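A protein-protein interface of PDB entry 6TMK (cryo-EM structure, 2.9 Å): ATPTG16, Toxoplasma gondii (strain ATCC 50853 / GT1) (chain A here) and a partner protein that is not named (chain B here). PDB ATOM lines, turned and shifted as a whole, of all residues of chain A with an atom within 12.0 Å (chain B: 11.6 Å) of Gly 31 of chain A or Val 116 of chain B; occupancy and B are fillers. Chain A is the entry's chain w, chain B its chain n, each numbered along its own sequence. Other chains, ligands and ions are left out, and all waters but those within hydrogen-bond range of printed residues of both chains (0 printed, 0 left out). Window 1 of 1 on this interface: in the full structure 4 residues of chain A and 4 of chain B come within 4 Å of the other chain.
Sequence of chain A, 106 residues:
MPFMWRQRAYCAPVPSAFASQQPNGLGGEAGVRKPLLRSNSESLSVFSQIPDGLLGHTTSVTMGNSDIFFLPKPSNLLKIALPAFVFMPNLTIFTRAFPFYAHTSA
Printed residues of chain B within 4 Å of Val 32 of chain A: Asn 115 (3.8 Å). Arg 33 of chain A touches just these residues of chain B: Asn 115 (2.4 Å), Val 116 (2.8 Å) and Asp 117 (3.2 Å). Of the printed residues of chain B, Lys 34 of chain A touches Asn 115 (3.1 Å). Leu 106 of chain B touches none of the printed residues of chain A. No residue of chain A comes within 4 Å of Lys 111 of chain B. Of chain A, only Val 32 (3.8 Å), Arg 33 (2.4 Å) and Lys 34 (3.1 Å) come within 4 Å of Asn 115 of chain B. Of chain A, only Gly 31 (3.5 Å) and Arg 33 (2.8 Å) come within 4 Å of Val 116 of chain B. No residue of chain A comes within 4 Å of Thr 119 of chain B. Of chain A, only Gly 31 comes within 4 Å of Asp 120 of chain B.
OD1 of Asp 117 of chain B lies within salt-bridge range of NH1 of Arg 33 of chain A, at 3.4 Å. OD1 of Asn 115 of chain B lies within hydrogen-bond range of NH2 of Arg 33 of chain A, 2.4 Å away. O of Gly 31 of chain A is in hydrogen-bond range of N of Asp 117 of chain B (3.1 Å). O of Val 116 of chain B is in hydrogen-bond range of NH1 of Arg 33 of chain A. The side-chain amide nitrogen of Asn 115 of chain B is in hydrogen-bond range of the backbone carbonyl oxygen of Lys 34 of chain A (3.1 Å).
Gly 31 of chain A touches Val 116 of chain B (O to CA, 3.5 Å). Gly 31 of chain A touches Asp 120 of chain B. O of Asn 115 of chain B touches CG1 of Val 32 of chain A, at 3.8 Å.
The side-chain carboxylate (OD2) of Asp 120 of chain B lies close to the backbone NH (N) of Gly 122 of chain B, at 3.4 Å. The side-chain amide oxygen (OE1) of Gln 22 of chain A sits close to the guanidinium group (NE) of Arg 33 of chain A, at 3.4 Å. NE2 of Gln 22 of chain A is in hydrogen-bond range of O of Lys 34 of chain A (3.2 Å). OD1 of Asp 120 of chain B lies within hydrogen-bond range of ND1 of His 103 of chain B, 3.0 Å away.
Of the 23 printed residues of chain B, 4 touch a printed residue of chain A. Among the printed residues, Asp or Glu carboxylates within 4 Å of a Lys or Arg side-chain nitrogen of the other chain: Arg 33 of chain A with Asp 117 of chain B (3.4 Å).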
ATOM      1  N   GLN A  22      24.960 -40.203  18.586  1.00  0.00           N
ATOM      2  CA  GLN A  22      24.402 -39.392  17.515  1.00  0.00           C
ATOM      3  C   GLN A  22      25.504 -38.867  16.603  1.00  0.00           C
ATOM      4  O   GLN A  22      26.138 -39.633  15.876  1.00  0.00           O
ATOM      5  CB  GLN A  22      23.608 -38.225  18.095  1.00  0.00           C
ATOM      6  CG  GLN A  22      22.725 -37.514  17.089  1.00  0.00           C
ATOM      7  CD  GLN A  22      21.469 -36.942  17.720  1.00  0.00           C
ATOM      8  OE1 GLN A  22      21.443 -36.636  18.912  1.00  0.00           O
ATOM      9  NE2 GLN A  22      20.424 -36.782  16.917  1.00  0.00           N
ATOM     10  N   GLY A  31      18.042 -26.528  17.381  1.00  0.00           N
ATOM     11  CA  GLY A  31      16.809 -26.718  18.123  1.00  0.00           C
ATOM     12  C   GLY A  31      16.408 -28.173  18.244  1.00  0.00           C
ATOM     13  O   GLY A  31      16.707 -28.834  19.236  1.00  0.00           O
ATOM     14  N   VAL A  32      15.720 -28.665  17.227  1.00  0.00           N
ATOM     15  CA  VAL A  32      15.246 -30.043  17.183  1.00  0.00           C
ATOM     16  C   VAL A  32      16.326 -30.924  16.578  1.00  0.00           C
ATOM     17  O   VAL A  32      16.994 -30.540  15.612  1.00  0.00           O
ATOM     18  CB  VAL A  32      13.936 -30.147  16.386  1.00  0.00           C
ATOM     19  CG1 VAL A  32      13.355 -31.539  16.509  1.00  0.00           C
ATOM     20  CG2 VAL A  32      12.954 -29.108  16.860  1.00  0.00           C
ATOM     21  N   ARG A  33      16.494 -32.113  17.143  1.00  0.00           N
ATOM     22  CA  ARG A  33      17.480 -33.063  16.657  1.00  0.00           C
ATOM     23  C   ARG A  33      16.856 -34.033  15.662  1.00  0.00           C
ATOM     24  O   ARG A  33      15.637 -34.181  15.576  1.00  0.00           O
ATOM     25  CB  ARG A  33      18.088 -33.843  17.819  1.00  0.00           C
ATOM     26  CG  ARG A  33      18.787 -32.997  18.853  1.00  0.00           C
ATOM     27  CD  ARG A  33      19.724 -33.845  19.687  1.00  0.00           C
ATOM     28  NE  ARG A  33      19.002 -34.849  20.463  1.00  0.00           N
ATOM     29  CZ  ARG A  33      18.668 -34.723  21.744  1.00  0.00           C
ATOM     30  NH1 ARG A  33      18.982 -33.626  22.421  1.00  0.00           N
ATOM     31  NH2 ARG A  33      18.005 -35.696  22.354  1.00  0.00           N
ATOM     32  N   LYS A  34      17.719 -34.694  14.902  1.00  0.00           N
ATOM     33  CA  LYS A  34      17.266 -35.721  13.985  1.00  0.00           C
ATOM     34  C   LYS A  34      16.908 -36.995  14.743  1.00  0.00           C
ATOM     35  O   LYS A  34      17.456 -37.263  15.815  1.00  0.00           O
ATOM     36  CB  LYS A  34      18.358 -36.023  12.968  1.00  0.00           C
ATOM     37  CG  LYS A  34      18.479 -34.982  11.872  1.00  0.00           C
ATOM     38  CD  LYS A  34      19.752 -35.152  11.066  1.00  0.00           C
ATOM     39  CE  LYS A  34      19.666 -36.325  10.107  1.00  0.00           C
ATOM     40  NZ  LYS A  34      18.837 -35.975   8.925  1.00  0.00           N
ATOM     41  N   PRO A  35      15.995 -37.802  14.212  1.00  0.00           N
ATOM     42  CA  PRO A  35      15.594 -39.016  14.923  1.00  0.00           C
ATOM     43  C   PRO A  35      16.730 -40.018  15.033  1.00  0.00           C
ATOM     44  O   PRO A  35      17.612 -40.098  14.176  1.00  0.00           O
ATOM     45  CB  PRO A  35      14.444 -39.562  14.071  1.00  0.00           C
ATOM     46  CG  PRO A  35      14.644 -38.968  12.739  1.00  0.00           C
ATOM     47  CD  PRO A  35      15.204 -37.611  12.987  1.00  0.00           C
ATOM     48  N   LEU A  36      16.690 -40.796  16.111  1.00  0.00           N
ATOM     49  CA  LEU A  36      17.734 -41.769  16.393  1.00  0.00           C
ATOM     50  C   LEU A  36      17.501 -43.093  15.689  1.00  0.00           C
ATOM     51  O   LEU A  36      18.461 -43.754  15.281  1.00  0.00           O
ATOM     52  CB  LEU A  36      17.835 -42.002  17.899  1.00  0.00           C
ATOM     53  CG  LEU A  36      17.955 -40.745  18.748  1.00  0.00           C
ATOM     54  CD1 LEU A  36      17.901 -41.107  20.202  1.00  0.00           C
ATOM     55  CD2 LEU A  36      19.229 -40.008  18.434  1.00  0.00           C
ATOM     56  N   HIS B  91       3.036 -28.236  27.690  1.00  0.00           N
ATOM     57  CA  HIS B  91       4.423 -28.562  27.387  1.00  0.00           C
ATOM     58  C   HIS B  91       5.025 -27.543  26.433  1.00  0.00           C
ATOM     59  O   HIS B  91       6.175 -27.127  26.600  1.00  0.00           O
ATOM     60  CB  HIS B  91       4.516 -29.956  26.773  1.00  0.00           C
ATOM     61  CG  HIS B  91       4.031 -31.050  27.667  1.00  0.00           C
ATOM     62  ND1 HIS B  91       4.004 -32.370  27.273  1.00  0.00           N
ATOM     63  CD2 HIS B  91       3.551 -31.024  28.931  1.00  0.00           C
ATOM     64  CE1 HIS B  91       3.528 -33.110  28.258  1.00  0.00           C
ATOM     65  NE2 HIS B  91       3.246 -32.318  29.276  1.00  0.00           N
ATOM     66  N   LEU B  92       4.250 -27.132  25.437  1.00  0.00           N
ATOM     67  CA  LEU B  92       4.689 -26.224  24.391  1.00  0.00           C
ATOM     68  C   LEU B  92       3.906 -24.927  24.512  1.00  0.00           C
ATOM     69  O   LEU B  92       2.678 -24.951  24.644  1.00  0.00           O
ATOM     70  CB  LEU B  92       4.480 -26.852  23.015  1.00  0.00           C
ATOM     71  CG  LEU B  92       4.973 -26.069  21.808  1.00  0.00           C
ATOM     72  CD1 LEU B  92       6.463 -26.214  21.677  1.00  0.00           C
ATOM     73  CD2 LEU B  92       4.287 -26.561  20.560  1.00  0.00           C
ATOM     74  N   HIS B 103       8.383 -17.037  18.820  1.00  0.00           N
ATOM     75  CA  HIS B 103       9.043 -18.329  18.776  1.00  0.00           C
ATOM     76  C   HIS B 103       8.216 -19.351  19.538  1.00  0.00           C
ATOM     77  O   HIS B 103       7.454 -19.006  20.442  1.00  0.00           O
ATOM     78  CB  HIS B 103      10.454 -18.258  19.361  1.00  0.00           C
ATOM     79  CG  HIS B 103      11.481 -17.772  18.389  1.00  0.00           C
ATOM     80  ND1 HIS B 103      12.733 -18.336  18.287  1.00  0.00           N
ATOM     81  CD2 HIS B 103      11.439 -16.780  17.470  1.00  0.00           C
ATOM     82  CE1 HIS B 103      13.421 -17.708  17.351  1.00  0.00           C
ATOM     83  NE2 HIS B 103      12.658 -16.761  16.839  1.00  0.00           N
ATOM     84  N   TYR B 104       8.341 -20.611  19.141  1.00  0.00           N
ATOM     85  CA  TYR B 104       7.775 -21.702  19.912  1.00  0.00           C
ATOM     86  C   TYR B 104       8.796 -22.111  20.962  1.00  0.00           C
ATOM     87  O   TYR B 104       9.983 -22.255  20.655  1.00  0.00           O
ATOM     88  CB  TYR B 104       7.422 -22.895  19.026  1.00  0.00           C
ATOM     89  CG  TYR B 104       6.059 -22.826  18.384  1.00  0.00           C
ATOM     90  CD1 TYR B 104       4.918 -22.668  19.151  1.00  0.00           C
ATOM     91  CD2 TYR B 104       5.910 -22.947  17.013  1.00  0.00           C
ATOM     92  CE1 TYR B 104       3.674 -22.610  18.572  1.00  0.00           C
ATOM     93  CE2 TYR B 104       4.668 -22.893  16.425  1.00  0.00           C
ATOM     94  CZ  TYR B 104       3.553 -22.729  17.210  1.00  0.00           C
ATOM     95  OH  TYR B 104       2.310 -22.674  16.626  1.00  0.00           O
ATOM     96  N   GLU B 105       8.338 -22.301  22.193  1.00  0.00           N
ATOM     97  CA  GLU B 105       9.217 -22.628  23.299  1.00  0.00           C
ATOM     98  C   GLU B 105       8.686 -23.849  24.025  1.00  0.00           C
ATOM     99  O   GLU B 105       7.481 -24.111  24.053  1.00  0.00           O
ATOM    100  CB  GLU B 105       9.351 -21.462  24.281  1.00  0.00           C
ATOM    101  CG  GLU B 105      10.480 -20.509  23.953  1.00  0.00           C
ATOM    102  CD  GLU B 105      10.853 -19.618  25.121  1.00  0.00           C
ATOM    103  OE1 GLU B 105      11.006 -20.141  26.244  1.00  0.00           O
ATOM    104  OE2 GLU B 105      10.994 -18.394  24.914  1.00  0.00           O
ATOM    105  N   LEU B 106       9.611 -24.599  24.605  1.00  0.00           N
ATOM    106  CA  LEU B 106       9.304 -25.819  25.323  1.00  0.00           C
ATOM    107  C   LEU B 106       9.684 -25.643  26.784  1.00  0.00           C
ATOM    108  O   LEU B 106      10.750 -25.101  27.095  1.00  0.00           O
ATOM    109  CB  LEU B 106      10.057 -26.999  24.711  1.00  0.00           C
ATOM    110  CG  LEU B 106       9.689 -28.402  25.159  1.00  0.00           C
ATOM    111  CD1 LEU B 106       8.379 -28.831  24.548  1.00  0.00           C
ATOM    112  CD2 LEU B 106      10.794 -29.332  24.750  1.00  0.00           C
ATOM    113  N   ARG B 107       8.812 -26.089  27.678  1.00  0.00           N
ATOM    114  CA  ARG B 107       9.095 -25.966  29.094  1.00  0.00           C
ATOM    115  C   ARG B 107      10.286 -26.851  29.457  1.00  0.00           C
ATOM    116  O   ARG B 107      10.547 -27.857  28.795  1.00  0.00           O
ATOM    117  CB  ARG B 107       7.881 -26.354  29.926  1.00  0.00           C
ATOM    118  CG  ARG B 107       6.632 -25.550  29.612  1.00  0.00           C
ATOM    119  CD  ARG B 107       6.770 -24.090  30.007  1.00  0.00           C
ATOM    120  NE  ARG B 107       7.172 -23.920  31.400  1.00  0.00           N
ATOM    121  CZ  ARG B 107       6.392 -24.193  32.442  1.00  0.00           C
ATOM    122  NH1 ARG B 107       5.157 -24.639  32.254  1.00  0.00           N
ATOM    123  NH2 ARG B 107       6.845 -24.010  33.675  1.00  0.00           N
ATOM    124  N   PRO B 108      11.023 -26.500  30.504  1.00  0.00           N
ATOM    125  CA  PRO B 108      12.218 -27.277  30.849  1.00  0.00           C
ATOM    126  C   PRO B 108      11.905 -28.603  31.519  1.00  0.00           C
ATOM    127  O   PRO B 108      12.616 -29.590  31.305  1.00  0.00           O
ATOM    128  CB  PRO B 108      12.972 -26.335  31.794  1.00  0.00           C
ATOM    129  CG  PRO B 108      11.893 -25.550  32.445  1.00  0.00           C
ATOM    130  CD  PRO B 108      10.866 -25.325  31.376  1.00  0.00           C
ATOM    131  N   GLU B 109      10.852 -28.647  32.334  1.00  0.00           N
ATOM    132  CA  GLU B 109      10.569 -29.844  33.112  1.00  0.00           C
ATOM    133  C   GLU B 109      10.061 -30.997  32.257  1.00  0.00           C
ATOM    134  O   GLU B 109       9.980 -32.125  32.756  1.00  0.00           O
ATOM    135  CB  GLU B 109       9.549 -29.529  34.205  1.00  0.00           C
ATOM    136  CG  GLU B 109       8.242 -28.961  33.691  1.00  0.00           C
ATOM    137  CD  GLU B 109       8.166 -27.455  33.829  1.00  0.00           C
ATOM    138  OE1 GLU B 109       9.198 -26.786  33.619  1.00  0.00           O
ATOM    139  OE2 GLU B 109       7.073 -26.941  34.146  1.00  0.00           O
ATOM    140  N   VAL B 110       9.716 -30.745  30.997  1.00  0.00           N
ATOM    141  CA  VAL B 110       9.338 -31.788  30.053  1.00  0.00           C
ATOM    142  C   VAL B 110      10.335 -31.885  28.902  1.00  0.00           C
ATOM    143  O   VAL B 110      10.023 -32.437  27.857  1.00  0.00           O
ATOM    144  CB  VAL B 110       7.907 -31.569  29.530  1.00  0.00           C
ATOM    145  CG1 VAL B 110       6.945 -31.429  30.684  1.00  0.00           C
ATOM    146  CG2 VAL B 110       7.851 -30.351  28.644  1.00  0.00           C
ATOM    147  N   LYS B 111      11.542 -31.352  29.089  1.00  0.00           N
ATOM    148  CA  LYS B 111      12.529 -31.386  28.019  1.00  0.00           C
ATOM    149  C   LYS B 111      13.036 -32.799  27.775  1.00  0.00           C
ATOM    150  O   LYS B 111      13.468 -33.118  26.661  1.00  0.00           O
ATOM    151  CB  LYS B 111      13.690 -30.456  28.355  1.00  0.00           C
ATOM    152  CG  LYS B 111      14.567 -30.117  27.174  1.00  0.00           C
ATOM    153  CD  LYS B 111      15.786 -29.324  27.597  1.00  0.00           C
ATOM    154  CE  LYS B 111      16.883 -30.237  28.118  1.00  0.00           C
ATOM    155  NZ  LYS B 111      17.543 -31.003  27.033  1.00  0.00           N
ATOM    156  N   HIS B 112      13.001 -33.654  28.796  1.00  0.00           N
ATOM    157  CA  HIS B 112      13.488 -35.017  28.658  1.00  0.00           C
ATOM    158  C   HIS B 112      12.540 -35.902  27.860  1.00  0.00           C
ATOM    159  O   HIS B 112      12.924 -37.018  27.496  1.00  0.00           O
ATOM    160  CB  HIS B 112      13.716 -35.621  30.040  1.00  0.00           C
ATOM    161  CG  HIS B 112      12.455 -35.886  30.797  1.00  0.00           C
ATOM    162  ND1 HIS B 112      11.720 -34.884  31.392  1.00  0.00           N
ATOM    163  CD2 HIS B 112      11.800 -37.040  31.062  1.00  0.00           C
ATOM    164  CE1 HIS B 112      10.665 -35.409  31.988  1.00  0.00           C
ATOM    165  NE2 HIS B 112      10.691 -36.717  31.802  1.00  0.00           N
ATOM    166  N   LEU B 113      11.323 -35.439  27.584  1.00  0.00           N
ATOM    167  CA  LEU B 113      10.392 -36.184  26.752  1.00  0.00           C
ATOM    168  C   LEU B 113      10.574 -35.903  25.270  1.00  0.00           C
ATOM    169  O   LEU B 113      10.063 -36.664  24.442  1.00  0.00           O
ATOM    170  CB  LEU B 113       8.948 -35.862  27.138  1.00  0.00           C
ATOM    171  CG  LEU B 113       8.525 -36.167  28.570  1.00  0.00           C
ATOM    172  CD1 LEU B 113       7.128 -35.641  28.789  1.00  0.00           C
ATOM    173  CD2 LEU B 113       8.593 -37.648  28.865  1.00  0.00           C
ATOM    174  N   TYR B 114      11.271 -34.828  24.923  1.00  0.00           N
ATOM    175  CA  TYR B 114      11.402 -34.388  23.547  1.00  0.00           C
ATOM    176  C   TYR B 114      12.854 -34.486  23.110  1.00  0.00           C
ATOM    177  O   TYR B 114      13.776 -34.354  23.920  1.00  0.00           O
ATOM    178  CB  TYR B 114      10.894 -32.959  23.385  1.00  0.00           C
ATOM    179  CG  TYR B 114       9.412 -32.833  23.625  1.00  0.00           C
ATOM    180  CD1 TYR B 114       8.507 -33.058  22.608  1.00  0.00           C
ATOM    181  CD2 TYR B 114       8.921 -32.508  24.875  1.00  0.00           C
ATOM    182  CE1 TYR B 114       7.161 -32.953  22.824  1.00  0.00           C
ATOM    183  CE2 TYR B 114       7.576 -32.401  25.099  1.00  0.00           C
ATOM    184  CZ  TYR B 114       6.696 -32.625  24.070  1.00  0.00           C
ATOM    185  OH  TYR B 114       5.342 -32.520  24.285  1.00  0.00           O
ATOM    186  N   ASN B 115      13.044 -34.723  21.814  1.00  0.00           N
ATOM    187  CA  ASN B 115      14.373 -34.885  21.233  1.00  0.00           C
ATOM    188  C   ASN B 115      14.861 -33.519  20.766  1.00  0.00           C
ATOM    189  O   ASN B 115      14.797 -33.161  19.590  1.00  0.00           O
ATOM    190  CB  ASN B 115      14.334 -35.897  20.099  1.00  0.00           C
ATOM    191  CG  ASN B 115      15.699 -36.411  19.733  1.00  0.00           C
ATOM    192  OD1 ASN B 115      16.578 -36.543  20.583  1.00  0.00           O
ATOM    193  ND2 ASN B 115      15.887 -36.716  18.463  1.00  0.00           N
ATOM    194  N   VAL B 116      15.358 -32.744  21.724  1.00  0.00           N
ATOM    195  CA  VAL B 116      15.802 -31.382  21.475  1.00  0.00           C
ATOM    196  C   VAL B 116      17.059 -31.102  22.281  1.00  0.00           C
ATOM    197  O   VAL B 116      17.267 -31.652  23.365  1.00  0.00           O
ATOM    198  CB  VAL B 116      14.710 -30.354  21.821  1.00  0.00           C
ATOM    199  CG1 VAL B 116      13.464 -30.641  21.038  1.00  0.00           C
ATOM    200  CG2 VAL B 116      14.427 -30.371  23.302  1.00  0.00           C
ATOM    201  N   ASP B 117      17.903 -30.235  21.728  1.00  0.00           N
ATOM    202  CA  ASP B 117      19.075 -29.764  22.451  1.00  0.00           C
ATOM    203  C   ASP B 117      18.712 -28.607  23.371  1.00  0.00           C
ATOM    204  O   ASP B 117      19.244 -28.497  24.481  1.00  0.00           O
ATOM    205  CB  ASP B 117      20.162 -29.343  21.465  1.00  0.00           C
ATOM    206  CG  ASP B 117      20.812 -30.526  20.773  1.00  0.00           C
ATOM    207  OD1 ASP B 117      21.401 -31.378  21.470  1.00  0.00           O
ATOM    208  OD2 ASP B 117      20.739 -30.601  19.528  1.00  0.00           O
ATOM    209  N   SER B 118      17.806 -27.740  22.925  1.00  0.00           N
ATOM    210  CA  SER B 118      17.379 -26.564  23.663  1.00  0.00           C
ATOM    211  C   SER B 118      15.857 -26.498  23.664  1.00  0.00           C
ATOM    212  O   SER B 118      15.172 -27.353  23.098  1.00  0.00           O
ATOM    213  CB  SER B 118      17.972 -25.288  23.060  1.00  0.00           C
ATOM    214  OG  SER B 118      17.895 -24.215  23.982  1.00  0.00           O
ATOM    215  N   THR B 119      15.331 -25.462  24.313  1.00  0.00           N
ATOM    216  CA  THR B 119      13.894 -25.248  24.396  1.00  0.00           C
ATOM    217  C   THR B 119      13.327 -24.507  23.197  1.00  0.00           C
ATOM    218  O   THR B 119      12.114 -24.565  22.971  1.00  0.00           O
ATOM    219  CB  THR B 119      13.552 -24.465  25.665  1.00  0.00           C
ATOM    220  OG1 THR B 119      14.269 -23.226  25.674  1.00  0.00           O
ATOM    221  CG2 THR B 119      13.921 -25.265  26.894  1.00  0.00           C
ATOM    222  N   ASP B 120      14.160 -23.809  22.432  1.00  0.00           N
ATOM    223  CA  ASP B 120      13.692 -23.028  21.294  1.00  0.00           C
ATOM    224  C   ASP B 120      13.495 -23.953  20.101  1.00  0.00           C
ATOM    225  O   ASP B 120      14.465 -24.478  19.545  1.00  0.00           O
ATOM    226  CB  ASP B 120      14.687 -21.920  20.966  1.00  0.00           C
ATOM    227  CG  ASP B 120      14.081 -20.826  20.114  1.00  0.00           C
ATOM    228  OD1 ASP B 120      14.833 -19.937  19.662  1.00  0.00           O
ATOM    229  OD2 ASP B 120      12.853 -20.850  19.894  1.00  0.00           O
ATOM    230  N   LEU B 121      12.240 -24.155  19.706  1.00  0.00           N
ATOM    231  CA  LEU B 121      11.896 -24.989  18.568  1.00  0.00           C
ATOM    232  C   LEU B 121      11.739 -24.194  17.280  1.00  0.00           C
ATOM    233  O   LEU B 121      11.176 -24.709  16.309  1.00  0.00           O
ATOM    234  CB  LEU B 121      10.615 -25.765  18.859  1.00  0.00           C
ATOM    235  CG  LEU B 121      10.596 -26.487  20.198  1.00  0.00           C
ATOM    236  CD1 LEU B 121       9.308 -27.233  20.346  1.00  0.00           C
ATOM    237  CD2 LEU B 121      11.773 -27.429  20.309  1.00  0.00           C
ATOM    238  N   GLY B 122      12.214 -22.959  17.253  1.00  0.00           N
ATOM    239  CA  GLY B 122      12.170 -22.142  16.059  1.00  0.00           C
ATOM    240  C   GLY B 122      10.981 -21.203  16.038  1.00  0.00           C
ATOM    241  O   GLY B 122      10.102 -21.219  16.904  1.00  0.00           O
ATOM    242  N   SER B 123      10.969 -20.374  15.000  1.00  0.00           N
ATOM    243  CA  SER B 123       9.941 -19.358  14.850  1.00  0.00           C
ATOM    244  C   SER B 123       8.578 -19.983  14.588  1.00  0.00           C
ATOM    245  O   SER B 123       8.465 -21.097  14.071  1.00  0.00           O
ATOM    246  CB  SER B 123      10.300 -18.414  13.708  1.00  0.00           C
ATOM    247  OG  SER B 123       9.154 -17.747  13.221  1.00  0.00           O
